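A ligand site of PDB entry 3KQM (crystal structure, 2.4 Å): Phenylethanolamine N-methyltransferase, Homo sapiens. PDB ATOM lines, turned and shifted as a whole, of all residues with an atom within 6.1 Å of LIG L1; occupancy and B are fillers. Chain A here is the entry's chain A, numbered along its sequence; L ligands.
The backbone carbonyl oxygen (O) of Phe 182 lies close to a sulfur (S1) of LIG L1, 3.6 Å away. Merely in contact with LIG L1: Tyr 27 (3.6 Å), Gly 81 (3.1 Å), Thr 83 (3.2 Å), Gln 86 (3.7 Å), Phe 102 (3.4 Å), Leu 103 (3.3 Å), Ile 157 (3.8 Å), His 160 (3.2 Å), Val 187 (3.3 Å) and Tyr 222 (3.9 Å). 22 residues have an atom within 4 Å of LIG L1: Tyr 27, Tyr 35, Tyr 40, Gly 79, Ser 80, Gly 81, Thr 83, Tyr 85, Gln 86, Asp 101, Phe 102, Leu 103, Asn 106, Ile 157, Asp 158, Val 159, His 160, Ala 181, Phe 182, Cys 183, Val 187 and Tyr 222. The nearest printed residue that does not touch LIG L1 is Ala 186 (4.2 Å).
The side-chain hydroxyl (OH) of Tyr 85 sits at hydrogen-bond distance from an oxygen (O1) of LIG L1. An oxygen (O2) of LIG L1 sits at hydrogen-bond distance from the side-chain hydroxyl (OH) of Tyr 40. O2 of LIG L1 lies within hydrogen-bond range of OH of Tyr 35 (2.6 Å). OD1 of Asp 101 sits at hydrogen-bond distance from O4 of LIG L1 (2.8 Å). N5 of LIG L1 is in hydrogen-bond range of N of Val 159, 2.8 Å away. A nitrogen (N1) of LIG L1 lies within hydrogen-bond range of the backbone carbonyl oxygen (O) of Gly 79 (2.8 Å). OD1 of Asn 106 is in hydrogen-bond range of O4 of LIG L1 (2.9 Å). N1 of LIG L1 sits at hydrogen-bond distance from O of Ala 181 (3.0 Å). N1 of LIG L1 lies within hydrogen-bond range of O of Ser 80 (3.2 Å). A nitrogen (N4) of LIG L1 sits at hydrogen-bond distance from the side-chain carboxylate (OD1) of Asp 158, at 3.3 Å. SG of Cys 183 is in hydrogen-bond range of N6 of LIG L1 (3.4 Å). The side-chain hydroxyl (OH) of Tyr 35 sits close to a nitrogen (N1) of LG2 L2 (3.3 Å). The side-chain amino group (NZ) of Lys 57 lies within hydrogen-bond range of a nitrogen (N2) of LG2 L2 (2.9 Å).
The side-chain hydroxyl of Tyr 85 sits at hydrogen-bond distance from the side-chain hydroxyl of Tyr 40. The side-chain hydroxyl (OH) of Tyr 40 sits at hydrogen-bond distance from the side-chain amino group (NZ) of Lys 57 (3.2 Å). The side-chain carboxylate (OD1) of Asp 101 sits at hydrogen-bond distance from the backbone NH (N) of Gly 81, at 3.1 Å. The side-chain carboxylate (OD2) of Asp 101 is in hydrogen-bond range of the backbone NH (N) of Leu 103 (3.0 Å). NE2 of Gln 86 lies within hydrogen-bond range of O of Ser 80. OH of Tyr 27 is in hydrogen-bond range of OH of Tyr 222 (3.0 Å). The backbone carbonyl oxygen (O) of Ala 186 sits at hydrogen-bond distance from the side-chain hydroxyl (OH) of Tyr 27 (2.4 Å). The side-chain carboxylate (OD2) of Asp 77 lies within hydrogen-bond range of the side-chain amide nitrogen (NE2) of Gln 86 (2.8 Å).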
ATOM      1  N   TYR A  27      12.770  19.002  11.397  1.00  0.00           N
ATOM      2  CA  TYR A  27      13.133  19.344  10.017  1.00  0.00           C
ATOM      3  C   TYR A  27      11.930  19.803   9.210  1.00  0.00           C
ATOM      4  O   TYR A  27      12.073  20.288   8.088  1.00  0.00           O
ATOM      5  CB  TYR A  27      13.904  18.213   9.312  1.00  0.00           C
ATOM      6  CG  TYR A  27      15.374  18.271   9.629  1.00  0.00           C
ATOM      7  CD1 TYR A  27      15.945  17.428  10.563  1.00  0.00           C
ATOM      8  CD2 TYR A  27      16.193  19.226   9.041  1.00  0.00           C
ATOM      9  CE1 TYR A  27      17.292  17.505  10.878  1.00  0.00           C
ATOM     10  CE2 TYR A  27      17.523  19.318   9.345  1.00  0.00           C
ATOM     11  CZ  TYR A  27      18.080  18.462  10.257  1.00  0.00           C
ATOM     12  OH  TYR A  27      19.418  18.567  10.548  1.00  0.00           O
ATOM     13  N   PHE A  30      12.133  23.519   9.056  1.00  0.00           N
ATOM     14  CA  PHE A  30      13.380  23.937   8.410  1.00  0.00           C
ATOM     15  C   PHE A  30      13.140  24.882   7.220  1.00  0.00           C
ATOM     16  O   PHE A  30      12.520  24.497   6.229  1.00  0.00           O
ATOM     17  CB  PHE A  30      14.135  22.677   7.956  1.00  0.00           C
ATOM     18  CG  PHE A  30      15.395  22.951   7.203  1.00  0.00           C
ATOM     19  CD1 PHE A  30      16.637  22.765   7.806  1.00  0.00           C
ATOM     20  CD2 PHE A  30      15.360  23.366   5.877  1.00  0.00           C
ATOM     21  CE1 PHE A  30      17.807  22.999   7.116  1.00  0.00           C
ATOM     22  CE2 PHE A  30      16.513  23.597   5.174  1.00  0.00           C
ATOM     23  CZ  PHE A  30      17.749  23.431   5.796  1.00  0.00           C
ATOM     24  N   TYR A  35      18.454  28.959   6.146  1.00  0.00           N
ATOM     25  CA  TYR A  35      19.647  28.150   6.223  1.00  0.00           C
ATOM     26  C   TYR A  35      20.755  28.706   5.325  1.00  0.00           C
ATOM     27  O   TYR A  35      21.894  28.876   5.764  1.00  0.00           O
ATOM     28  CB  TYR A  35      19.352  26.695   5.859  1.00  0.00           C
ATOM     29  CG  TYR A  35      20.573  25.803   5.876  1.00  0.00           C
ATOM     30  CD1 TYR A  35      21.061  25.276   7.071  1.00  0.00           C
ATOM     31  CD2 TYR A  35      21.229  25.470   4.688  1.00  0.00           C
ATOM     32  CE1 TYR A  35      22.164  24.445   7.086  1.00  0.00           C
ATOM     33  CE2 TYR A  35      22.352  24.631   4.707  1.00  0.00           C
ATOM     34  CZ  TYR A  35      22.811  24.135   5.902  1.00  0.00           C
ATOM     35  OH  TYR A  35      23.911  23.313   5.926  1.00  0.00           O
ATOM     36  N   ASN A  39      24.295  30.438   6.593  1.00  0.00           N
ATOM     37  CA  ASN A  39      25.475  29.613   6.351  1.00  0.00           C
ATOM     38  C   ASN A  39      26.311  29.946   5.132  1.00  0.00           C
ATOM     39  O   ASN A  39      27.507  29.661   5.107  1.00  0.00           O
ATOM     40  CB  ASN A  39      25.087  28.127   6.319  1.00  0.00           C
ATOM     41  CG  ASN A  39      24.686  27.613   7.676  1.00  0.00           C
ATOM     42  OD1 ASN A  39      25.473  27.618   8.613  1.00  0.00           O
ATOM     43  ND2 ASN A  39      23.443  27.161   7.782  1.00  0.00           N
ATOM     44  N   TYR A  40      25.693  30.551   4.127  1.00  0.00           N
ATOM     45  CA  TYR A  40      26.398  30.766   2.858  1.00  0.00           C
ATOM     46  C   TYR A  40      26.386  32.207   2.353  1.00  0.00           C
ATOM     47  O   TYR A  40      26.934  32.508   1.299  1.00  0.00           O
ATOM     48  CB  TYR A  40      25.895  29.772   1.817  1.00  0.00           C
ATOM     49  CG  TYR A  40      26.206  28.369   2.252  1.00  0.00           C
ATOM     50  CD1 TYR A  40      25.275  27.597   2.932  1.00  0.00           C
ATOM     51  CD2 TYR A  40      27.480  27.838   2.059  1.00  0.00           C
ATOM     52  CE1 TYR A  40      25.578  26.308   3.360  1.00  0.00           C
ATOM     53  CE2 TYR A  40      27.799  26.573   2.477  1.00  0.00           C
ATOM     54  CZ  TYR A  40      26.853  25.809   3.123  1.00  0.00           C
ATOM     55  OH  TYR A  40      27.195  24.547   3.525  1.00  0.00           O
ATOM     56  N   LYS A  57      36.225  24.891   2.767  1.00  0.00           N
ATOM     57  CA  LYS A  57      35.426  23.800   2.202  1.00  0.00           C
ATOM     58  C   LYS A  57      35.715  23.575   0.720  1.00  0.00           C
ATOM     59  O   LYS A  57      35.895  22.425   0.288  1.00  0.00           O
ATOM     60  CB  LYS A  57      33.931  24.051   2.400  1.00  0.00           C
ATOM     61  CG  LYS A  57      33.592  24.565   3.789  1.00  0.00           C
ATOM     62  CD  LYS A  57      32.260  24.053   4.278  1.00  0.00           C
ATOM     63  CE  LYS A  57      31.097  24.952   3.912  1.00  0.00           C
ATOM     64  NZ  LYS A  57      30.040  24.871   4.991  1.00  0.00           N
ATOM     65  N   ASP A  77      25.103  12.775  -4.246  1.00  0.00           N
ATOM     66  CA  ASP A  77      25.286  13.725  -3.155  1.00  0.00           C
ATOM     67  C   ASP A  77      24.202  13.491  -2.103  1.00  0.00           C
ATOM     68  O   ASP A  77      23.003  13.603  -2.406  1.00  0.00           O
ATOM     69  CB  ASP A  77      25.231  15.165  -3.687  1.00  0.00           C
ATOM     70  CG  ASP A  77      25.515  16.192  -2.610  1.00  0.00           C
ATOM     71  OD1 ASP A  77      26.182  15.853  -1.615  1.00  0.00           O
ATOM     72  OD2 ASP A  77      25.067  17.356  -2.764  1.00  0.00           O
ATOM     73  N   ILE A  78      24.622  13.162  -0.888  1.00  0.00           N
ATOM     74  CA  ILE A  78      23.690  12.788   0.178  1.00  0.00           C
ATOM     75  C   ILE A  78      23.344  13.979   1.061  1.00  0.00           C
ATOM     76  O   ILE A  78      24.226  14.579   1.671  1.00  0.00           O
ATOM     77  CB  ILE A  78      24.285  11.679   1.118  1.00  0.00           C
ATOM     78  CG1 ILE A  78      24.912  10.525   0.332  1.00  0.00           C
ATOM     79  CG2 ILE A  78      23.220  11.193   2.107  1.00  0.00           C
ATOM     80  CD1 ILE A  78      23.962   9.820  -0.618  1.00  0.00           C
ATOM     81  N   GLY A  79      22.055  14.285   1.168  1.00  0.00           N
ATOM     82  CA  GLY A  79      21.592  15.374   2.011  1.00  0.00           C
ATOM     83  C   GLY A  79      22.027  16.717   1.486  1.00  0.00           C
ATOM     84  O   GLY A  79      22.623  17.528   2.213  1.00  0.00           O
ATOM     85  N   SER A  80      21.738  16.967   0.211  1.00  0.00           N
ATOM     86  CA  SER A  80      22.199  18.165  -0.480  1.00  0.00           C
ATOM     87  C   SER A  80      21.655  19.451   0.131  1.00  0.00           C
ATOM     88  O   SER A  80      22.272  20.517   0.003  1.00  0.00           O
ATOM     89  CB  SER A  80      21.789  18.090  -1.953  1.00  0.00           C
ATOM     90  OG  SER A  80      22.329  16.941  -2.574  1.00  0.00           O
ATOM     91  N   GLY A  81      20.508  19.347   0.786  1.00  0.00           N
ATOM     92  CA  GLY A  81      19.775  20.524   1.209  1.00  0.00           C
ATOM     93  C   GLY A  81      19.584  21.435   0.010  1.00  0.00           C
ATOM     94  O   GLY A  81      19.344  20.972  -1.101  1.00  0.00           O
ATOM     95  N   PRO A  82      19.709  22.745   0.220  1.00  0.00           N
ATOM     96  CA  PRO A  82      19.491  23.693  -0.869  1.00  0.00           C
ATOM     97  C   PRO A  82      20.826  24.178  -1.436  1.00  0.00           C
ATOM     98  O   PRO A  82      20.855  25.247  -2.029  1.00  0.00           O
ATOM     99  CB  PRO A  82      18.814  24.871  -0.169  1.00  0.00           C
ATOM    100  CG  PRO A  82      19.185  24.723   1.336  1.00  0.00           C
ATOM    101  CD  PRO A  82      19.980  23.454   1.483  1.00  0.00           C
ATOM    102  N   THR A  83      21.905  23.433  -1.223  1.00  0.00           N
ATOM    103  CA  THR A  83      23.226  23.923  -1.630  1.00  0.00           C
ATOM    104  C   THR A  83      23.865  23.069  -2.735  1.00  0.00           C
ATOM    105  O   THR A  83      23.653  21.853  -2.778  1.00  0.00           O
ATOM    106  CB  THR A  83      24.196  24.125  -0.408  1.00  0.00           C
ATOM    107  OG1 THR A  83      24.788  22.880   0.002  1.00  0.00           O
ATOM    108  CG2 THR A  83      23.468  24.761   0.770  1.00  0.00           C
ATOM    109  N   TYR A  85      27.354  23.941  -3.826  1.00  0.00           N
ATOM    110  CA  TYR A  85      28.793  24.214  -3.805  1.00  0.00           C
ATOM    111  C   TYR A  85      29.581  22.932  -3.646  1.00  0.00           C
ATOM    112  O   TYR A  85      30.743  22.850  -4.063  1.00  0.00           O
ATOM    113  CB  TYR A  85      29.149  25.140  -2.637  1.00  0.00           C
ATOM    114  CG  TYR A  85      29.027  24.415  -1.302  1.00  0.00           C
ATOM    115  CD1 TYR A  85      30.122  23.769  -0.740  1.00  0.00           C
ATOM    116  CD2 TYR A  85      27.815  24.339  -0.637  1.00  0.00           C
ATOM    117  CE1 TYR A  85      30.020  23.094   0.452  1.00  0.00           C
ATOM    118  CE2 TYR A  85      27.701  23.662   0.562  1.00  0.00           C
ATOM    119  CZ  TYR A  85      28.807  23.040   1.092  1.00  0.00           C
ATOM    120  OH  TYR A  85      28.688  22.359   2.284  1.00  0.00           O
ATOM    121  N   GLN A  86      28.990  21.933  -3.002  1.00  0.00           N
ATOM    122  CA  GLN A  86      29.715  20.710  -2.683  1.00  0.00           C
ATOM    123  C   GLN A  86      29.994  19.855  -3.909  1.00  0.00           C
ATOM    124  O   GLN A  86      30.656  18.815  -3.811  1.00  0.00           O
ATOM    125  CB  GLN A  86      29.010  19.907  -1.577  1.00  0.00           C
ATOM    126  CG  GLN A  86      27.621  19.344  -1.930  1.00  0.00           C
ATOM    127  CD  GLN A  86      26.528  20.363  -1.693  1.00  0.00           C
ATOM    128  OE1 GLN A  86      26.797  21.573  -1.590  1.00  0.00           O
ATOM    129  NE2 GLN A  86      25.293  19.888  -1.593  1.00  0.00           N
ATOM    130  N   ASP A 101      17.681  15.070  -1.068  1.00  0.00           N
ATOM    131  CA  ASP A 101      17.384  15.567   0.279  1.00  0.00           C
ATOM    132  C   ASP A 101      16.076  15.041   0.814  1.00  0.00           C
ATOM    133  O   ASP A 101      15.170  14.691   0.065  1.00  0.00           O
ATOM    134  CB  ASP A 101      17.356  17.092   0.331  1.00  0.00           C
ATOM    135  CG  ASP A 101      17.554  17.606   1.735  1.00  0.00           C
ATOM    136  OD1 ASP A 101      18.666  17.412   2.266  1.00  0.00           O
ATOM    137  OD2 ASP A 101      16.595  18.199   2.286  1.00  0.00           O
ATOM    138  N   PHE A 102      15.993  15.005   2.140  1.00  0.00           N
ATOM    139  CA  PHE A 102      14.816  14.544   2.845  1.00  0.00           C
ATOM    140  C   PHE A 102      13.626  15.486   2.626  1.00  0.00           C
ATOM    141  O   PHE A 102      12.482  15.046   2.561  1.00  0.00           O
ATOM    142  CB  PHE A 102      15.132  14.411   4.335  1.00  0.00           C
ATOM    143  CG  PHE A 102      14.019  13.834   5.158  1.00  0.00           C
ATOM    144  CD1 PHE A 102      13.768  12.482   5.150  1.00  0.00           C
ATOM    145  CD2 PHE A 102      13.241  14.648   5.955  1.00  0.00           C
ATOM    146  CE1 PHE A 102      12.747  11.942   5.923  1.00  0.00           C
ATOM    147  CE2 PHE A 102      12.210  14.116   6.716  1.00  0.00           C
ATOM    148  CZ  PHE A 102      11.971  12.766   6.700  1.00  0.00           C
ATOM    149  N   LEU A 103      13.909  16.779   2.506  1.00  0.00           N
ATOM    150  CA  LEU A 103      12.853  17.791   2.400  1.00  0.00           C
ATOM    151  C   LEU A 103      12.563  18.240   0.975  1.00  0.00           C
ATOM    152  O   LEU A 103      13.458  18.598   0.212  1.00  0.00           O
ATOM    153  CB  LEU A 103      13.193  19.011   3.257  1.00  0.00           C
ATOM    154  CG  LEU A 103      13.216  18.755   4.772  1.00  0.00           C
ATOM    155  CD1 LEU A 103      13.838  19.937   5.495  1.00  0.00           C
ATOM    156  CD2 LEU A 103      11.810  18.444   5.297  1.00  0.00           C
ATOM    157  N   ASN A 106      13.640  21.807   0.071  1.00  0.00           N
ATOM    158  CA  ASN A 106      15.031  21.824  -0.357  1.00  0.00           C
ATOM    159  C   ASN A 106      15.187  21.380  -1.793  1.00  0.00           C
ATOM    160  O   ASN A 106      15.943  21.982  -2.558  1.00  0.00           O
ATOM    161  CB  ASN A 106      15.907  20.981   0.550  1.00  0.00           C
ATOM    162  CG  ASN A 106      16.454  21.758   1.714  1.00  0.00           C
ATOM    163  OD1 ASN A 106      17.110  21.204   2.604  1.00  0.00           O
ATOM    164  ND2 ASN A 106      16.198  23.057   1.732  1.00  0.00           N
ATOM    165  N   ILE A 157      15.311  11.164  -0.092  1.00  0.00           N
ATOM    166  CA  ILE A 157      16.281  10.313   0.569  1.00  0.00           C
ATOM    167  C   ILE A 157      16.105  10.370   2.092  1.00  0.00           C
ATOM    168  O   ILE A 157      15.799  11.427   2.651  1.00  0.00           O
ATOM    169  CB  ILE A 157      17.725  10.729   0.170  1.00  0.00           C
ATOM    170  CG1 ILE A 157      18.742   9.651   0.569  1.00  0.00           C
ATOM    171  CG2 ILE A 157      18.063  12.112   0.755  1.00  0.00           C
ATOM    172  CD1 ILE A 157      20.201  10.076   0.401  1.00  0.00           C
ATOM    173  N   ASP A 158      16.272   9.227   2.752  1.00  0.00           N
ATOM    174  CA  ASP A 158      16.206   9.178   4.204  1.00  0.00           C
ATOM    175  C   ASP A 158      17.299   8.235   4.688  1.00  0.00           C
ATOM    176  O   ASP A 158      17.194   7.011   4.521  1.00  0.00           O
ATOM    177  CB  ASP A 158      14.838   8.685   4.692  1.00  0.00           C
ATOM    178  CG  ASP A 158      14.791   8.473   6.198  1.00  0.00           C
ATOM    179  OD1 ASP A 158      15.869   8.464   6.839  1.00  0.00           O
ATOM    180  OD2 ASP A 158      13.673   8.300   6.744  1.00  0.00           O
ATOM    181  N   VAL A 159      18.343   8.806   5.282  1.00  0.00           N
ATOM    182  CA  VAL A 159      19.516   8.021   5.604  1.00  0.00           C
ATOM    183  C   VAL A 159      19.264   7.052   6.779  1.00  0.00           C
ATOM    184  O   VAL A 159      20.019   6.097   6.980  1.00  0.00           O
ATOM    185  CB  VAL A 159      20.748   8.916   5.864  1.00  0.00           C
ATOM    186  CG1 VAL A 159      20.986   9.818   4.671  1.00  0.00           C
ATOM    187  CG2 VAL A 159      20.549   9.733   7.128  1.00  0.00           C
ATOM    188  N   HIS A 160      18.203   7.287   7.528  1.00  0.00           N
ATOM    189  CA  HIS A 160      17.843   6.383   8.614  1.00  0.00           C
ATOM    190  C   HIS A 160      17.303   5.052   8.081  1.00  0.00           C
ATOM    191  O   HIS A 160      17.179   4.083   8.843  1.00  0.00           O
ATOM    192  CB  HIS A 160      16.857   7.037   9.561  1.00  0.00           C
ATOM    193  CG  HIS A 160      17.374   8.292  10.189  1.00  0.00           C
ATOM    194  ND1 HIS A 160      18.588   8.349  10.841  1.00  0.00           N
ATOM    195  CD2 HIS A 160      16.843   9.539  10.259  1.00  0.00           C
ATOM    196  CE1 HIS A 160      18.786   9.572  11.290  1.00  0.00           C
ATOM    197  NE2 HIS A 160      17.743  10.316  10.952  1.00  0.00           N
ATOM    198  N   SER A 180      28.803  13.952   0.772  1.00  0.00           N
ATOM    199  CA  SER A 180      27.793  14.338   1.741  1.00  0.00           C
ATOM    200  C   SER A 180      28.324  15.376   2.703  1.00  0.00           C
ATOM    201  O   SER A 180      29.323  15.137   3.392  1.00  0.00           O
ATOM    202  CB  SER A 180      27.294  13.129   2.527  1.00  0.00           C
ATOM    203  OG  SER A 180      26.345  13.550   3.492  1.00  0.00           O
ATOM    204  N   ALA A 181      27.652  16.516   2.762  1.00  0.00           N
ATOM    205  CA  ALA A 181      28.106  17.619   3.604  1.00  0.00           C
ATOM    206  C   ALA A 181      27.086  18.035   4.666  1.00  0.00           C
ATOM    207  O   ALA A 181      25.989  18.473   4.339  1.00  0.00           O
ATOM    208  CB  ALA A 181      28.481  18.818   2.731  1.00  0.00           C
ATOM    209  N   PHE A 182      27.481  17.903   5.927  1.00  0.00           N
ATOM    210  CA  PHE A 182      26.702  18.455   7.028  1.00  0.00           C
ATOM    211  C   PHE A 182      25.313  17.823   7.102  1.00  0.00           C
ATOM    212  O   PHE A 182      24.362  18.445   7.593  1.00  0.00           O
ATOM    213  CB  PHE A 182      26.608  19.972   6.903  1.00  0.00           C
ATOM    214  CG  PHE A 182      27.950  20.651   6.805  1.00  0.00           C
ATOM    215  CD1 PHE A 182      28.522  20.899   5.560  1.00  0.00           C
ATOM    216  CD2 PHE A 182      28.646  21.012   7.946  1.00  0.00           C
ATOM    217  CE1 PHE A 182      29.766  21.507   5.469  1.00  0.00           C
ATOM    218  CE2 PHE A 182      29.886  21.614   7.861  1.00  0.00           C
ATOM    219  CZ  PHE A 182      30.454  21.855   6.622  1.00  0.00           C
ATOM    220  N   CYS A 183      25.198  16.606   6.613  1.00  0.00           N
ATOM    221  CA  CYS A 183      23.971  15.843   6.716  1.00  0.00           C
ATOM    222  C   CYS A 183      23.944  14.931   7.944  1.00  0.00           C
ATOM    223  O   CYS A 183      23.245  15.211   8.916  1.00  0.00           O
ATOM    224  CB  CYS A 183      23.745  15.002   5.461  1.00  0.00           C
ATOM    225  SG  CYS A 183      22.176  14.113   5.476  1.00  0.00           S
ATOM    226  N   LEU A 184      24.715  13.839   7.902  1.00  0.00           N
ATOM    227  CA  LEU A 184      24.650  12.805   8.937  1.00  0.00           C
ATOM    228  C   LEU A 184      24.593  13.333  10.382  1.00  0.00           C
ATOM    229  O   LEU A 184      23.630  13.085  11.099  1.00  0.00           O
ATOM    230  CB  LEU A 184      25.808  11.813   8.802  1.00  0.00           C
ATOM    231  CG  LEU A 184      26.007  11.207   7.419  1.00  0.00           C
ATOM    232  CD1 LEU A 184      26.887   9.976   7.546  1.00  0.00           C
ATOM    233  CD2 LEU A 184      24.676  10.851   6.799  1.00  0.00           C
ATOM    234  N   ALA A 186      23.911  16.057  11.484  1.00  0.00           N
ATOM    235  CA  ALA A 186      22.781  16.968  11.674  1.00  0.00           C
ATOM    236  C   ALA A 186      21.407  16.279  11.707  1.00  0.00           C
ATOM    237  O   ALA A 186      20.414  16.916  12.059  1.00  0.00           O
ATOM    238  CB  ALA A 186      22.802  18.060  10.581  1.00  0.00           C
ATOM    239  N   VAL A 187      21.348  15.005  11.332  1.00  0.00           N
ATOM    240  CA  VAL A 187      20.090  14.260  11.340  1.00  0.00           C
ATOM    241  C   VAL A 187      20.097  13.106  12.347  1.00  0.00           C
ATOM    242  O   VAL A 187      19.172  12.297  12.386  1.00  0.00           O
ATOM    243  CB  VAL A 187      19.774  13.662   9.950  1.00  0.00           C
ATOM    244  CG1 VAL A 187      19.667  14.753   8.909  1.00  0.00           C
ATOM    245  CG2 VAL A 187      20.816  12.616   9.553  1.00  0.00           C
ATOM    246  N   TYR A 222      21.735  23.935  15.485  1.00  0.00           N
ATOM    247  CA  TYR A 222      21.790  25.089  14.596  1.00  0.00           C
ATOM    248  C   TYR A 222      20.367  25.500  14.220  1.00  0.00           C
ATOM    249  O   TYR A 222      19.419  24.705  14.342  1.00  0.00           O
ATOM    250  CB  TYR A 222      22.617  24.806  13.341  1.00  0.00           C
ATOM    251  CG  TYR A 222      21.956  23.864  12.377  1.00  0.00           C
ATOM    252  CD1 TYR A 222      21.250  24.352  11.283  1.00  0.00           C
ATOM    253  CD2 TYR A 222      22.024  22.474  12.549  1.00  0.00           C
ATOM    254  CE1 TYR A 222      20.643  23.484  10.387  1.00  0.00           C
ATOM    255  CE2 TYR A 222      21.409  21.612  11.655  1.00  0.00           C
ATOM    256  CZ  TYR A 222      20.729  22.130  10.580  1.00  0.00           C
ATOM    257  OH  TYR A 222      20.113  21.305   9.679  1.00  0.00           O
HETATM  258  N1  LIG L   1      24.528  19.627   2.014  1.00  0.00           N
HETATM  259  C1  LIG L   1      24.036  20.797   2.737  1.00  0.00           C
HETATM  260  C2  LIG L   1      23.580  20.302   4.131  1.00  0.00           C
HETATM  261  C3  LIG L   1      22.143  20.736   4.409  1.00  0.00           C
HETATM  262  S1  LIG L   1      21.917  20.746   6.222  1.00  0.00           S
HETATM  263  C4  LIG L   1      25.235  21.752   2.932  1.00  0.00           C
HETATM  264  O1  LIG L   1      26.341  21.304   2.846  1.00  0.00           O
HETATM  265  O2  LIG L   1      25.056  22.988   3.560  1.00  0.00           O
HETATM  266  C5  LIG L   1      21.308  19.106   6.745  1.00  0.00           C
HETATM  267  C6  LIG L   1      20.435  18.479   5.654  1.00  0.00           C
HETATM  268  O3  LIG L   1      20.013  17.131   6.018  1.00  0.00           O
HETATM  269  C7  LIG L   1      19.143  19.273   5.385  1.00  0.00           C
HETATM  270  O4  LIG L   1      19.031  19.540   4.008  1.00  0.00           O
HETATM  271  C8  LIG L   1      18.080  18.300   5.805  1.00  0.00           C
HETATM  272  O5  LIG L   1      16.807  18.521   5.239  1.00  0.00           O
HETATM  273  C9  LIG L   1      18.684  16.962   5.433  1.00  0.00           C
HETATM  274  N2  LIG L   1      17.984  15.911   6.146  1.00  0.00           N
HETATM  275  C10 LIG L   1      17.064  16.106   7.311  1.00  0.00           C
HETATM  276  N3  LIG L   1      16.615  14.784   7.754  1.00  0.00           N
HETATM  277  C11 LIG L   1      17.265  13.791   6.888  1.00  0.00           C
HETATM  278  C12 LIG L   1      17.177  12.286   6.869  1.00  0.00           C
HETATM  279  N4  LIG L   1      16.340  11.615   7.851  1.00  0.00           N
HETATM  280  N5  LIG L   1      17.938  11.538   5.876  1.00  0.00           N
HETATM  281  C13 LIG L   1      18.802  12.255   4.866  1.00  0.00           C
HETATM  282  N6  LIG L   1      18.869  13.750   4.877  1.00  0.00           N
HETATM  283  C14 LIG L   1      18.110  14.493   5.898  1.00  0.00           C
HETATM  284 BR1  LG2 L   2      29.907  25.314   9.144  1.00  0.00          BR
HETATM  285  C1  LG2 L   2      28.282  24.568   8.376  1.00  0.00           C
HETATM  286  C2  LG2 L   2      27.190  24.106   9.082  1.00  0.00           C
HETATM  287  N1  LG2 L   2      26.262  23.694   8.200  1.00  0.00           N
HETATM  288  C3  LG2 L   2      26.768  23.923   6.941  1.00  0.00           C
HETATM  289  N2  LG2 L   2      28.021  24.467   7.061  1.00  0.00           N
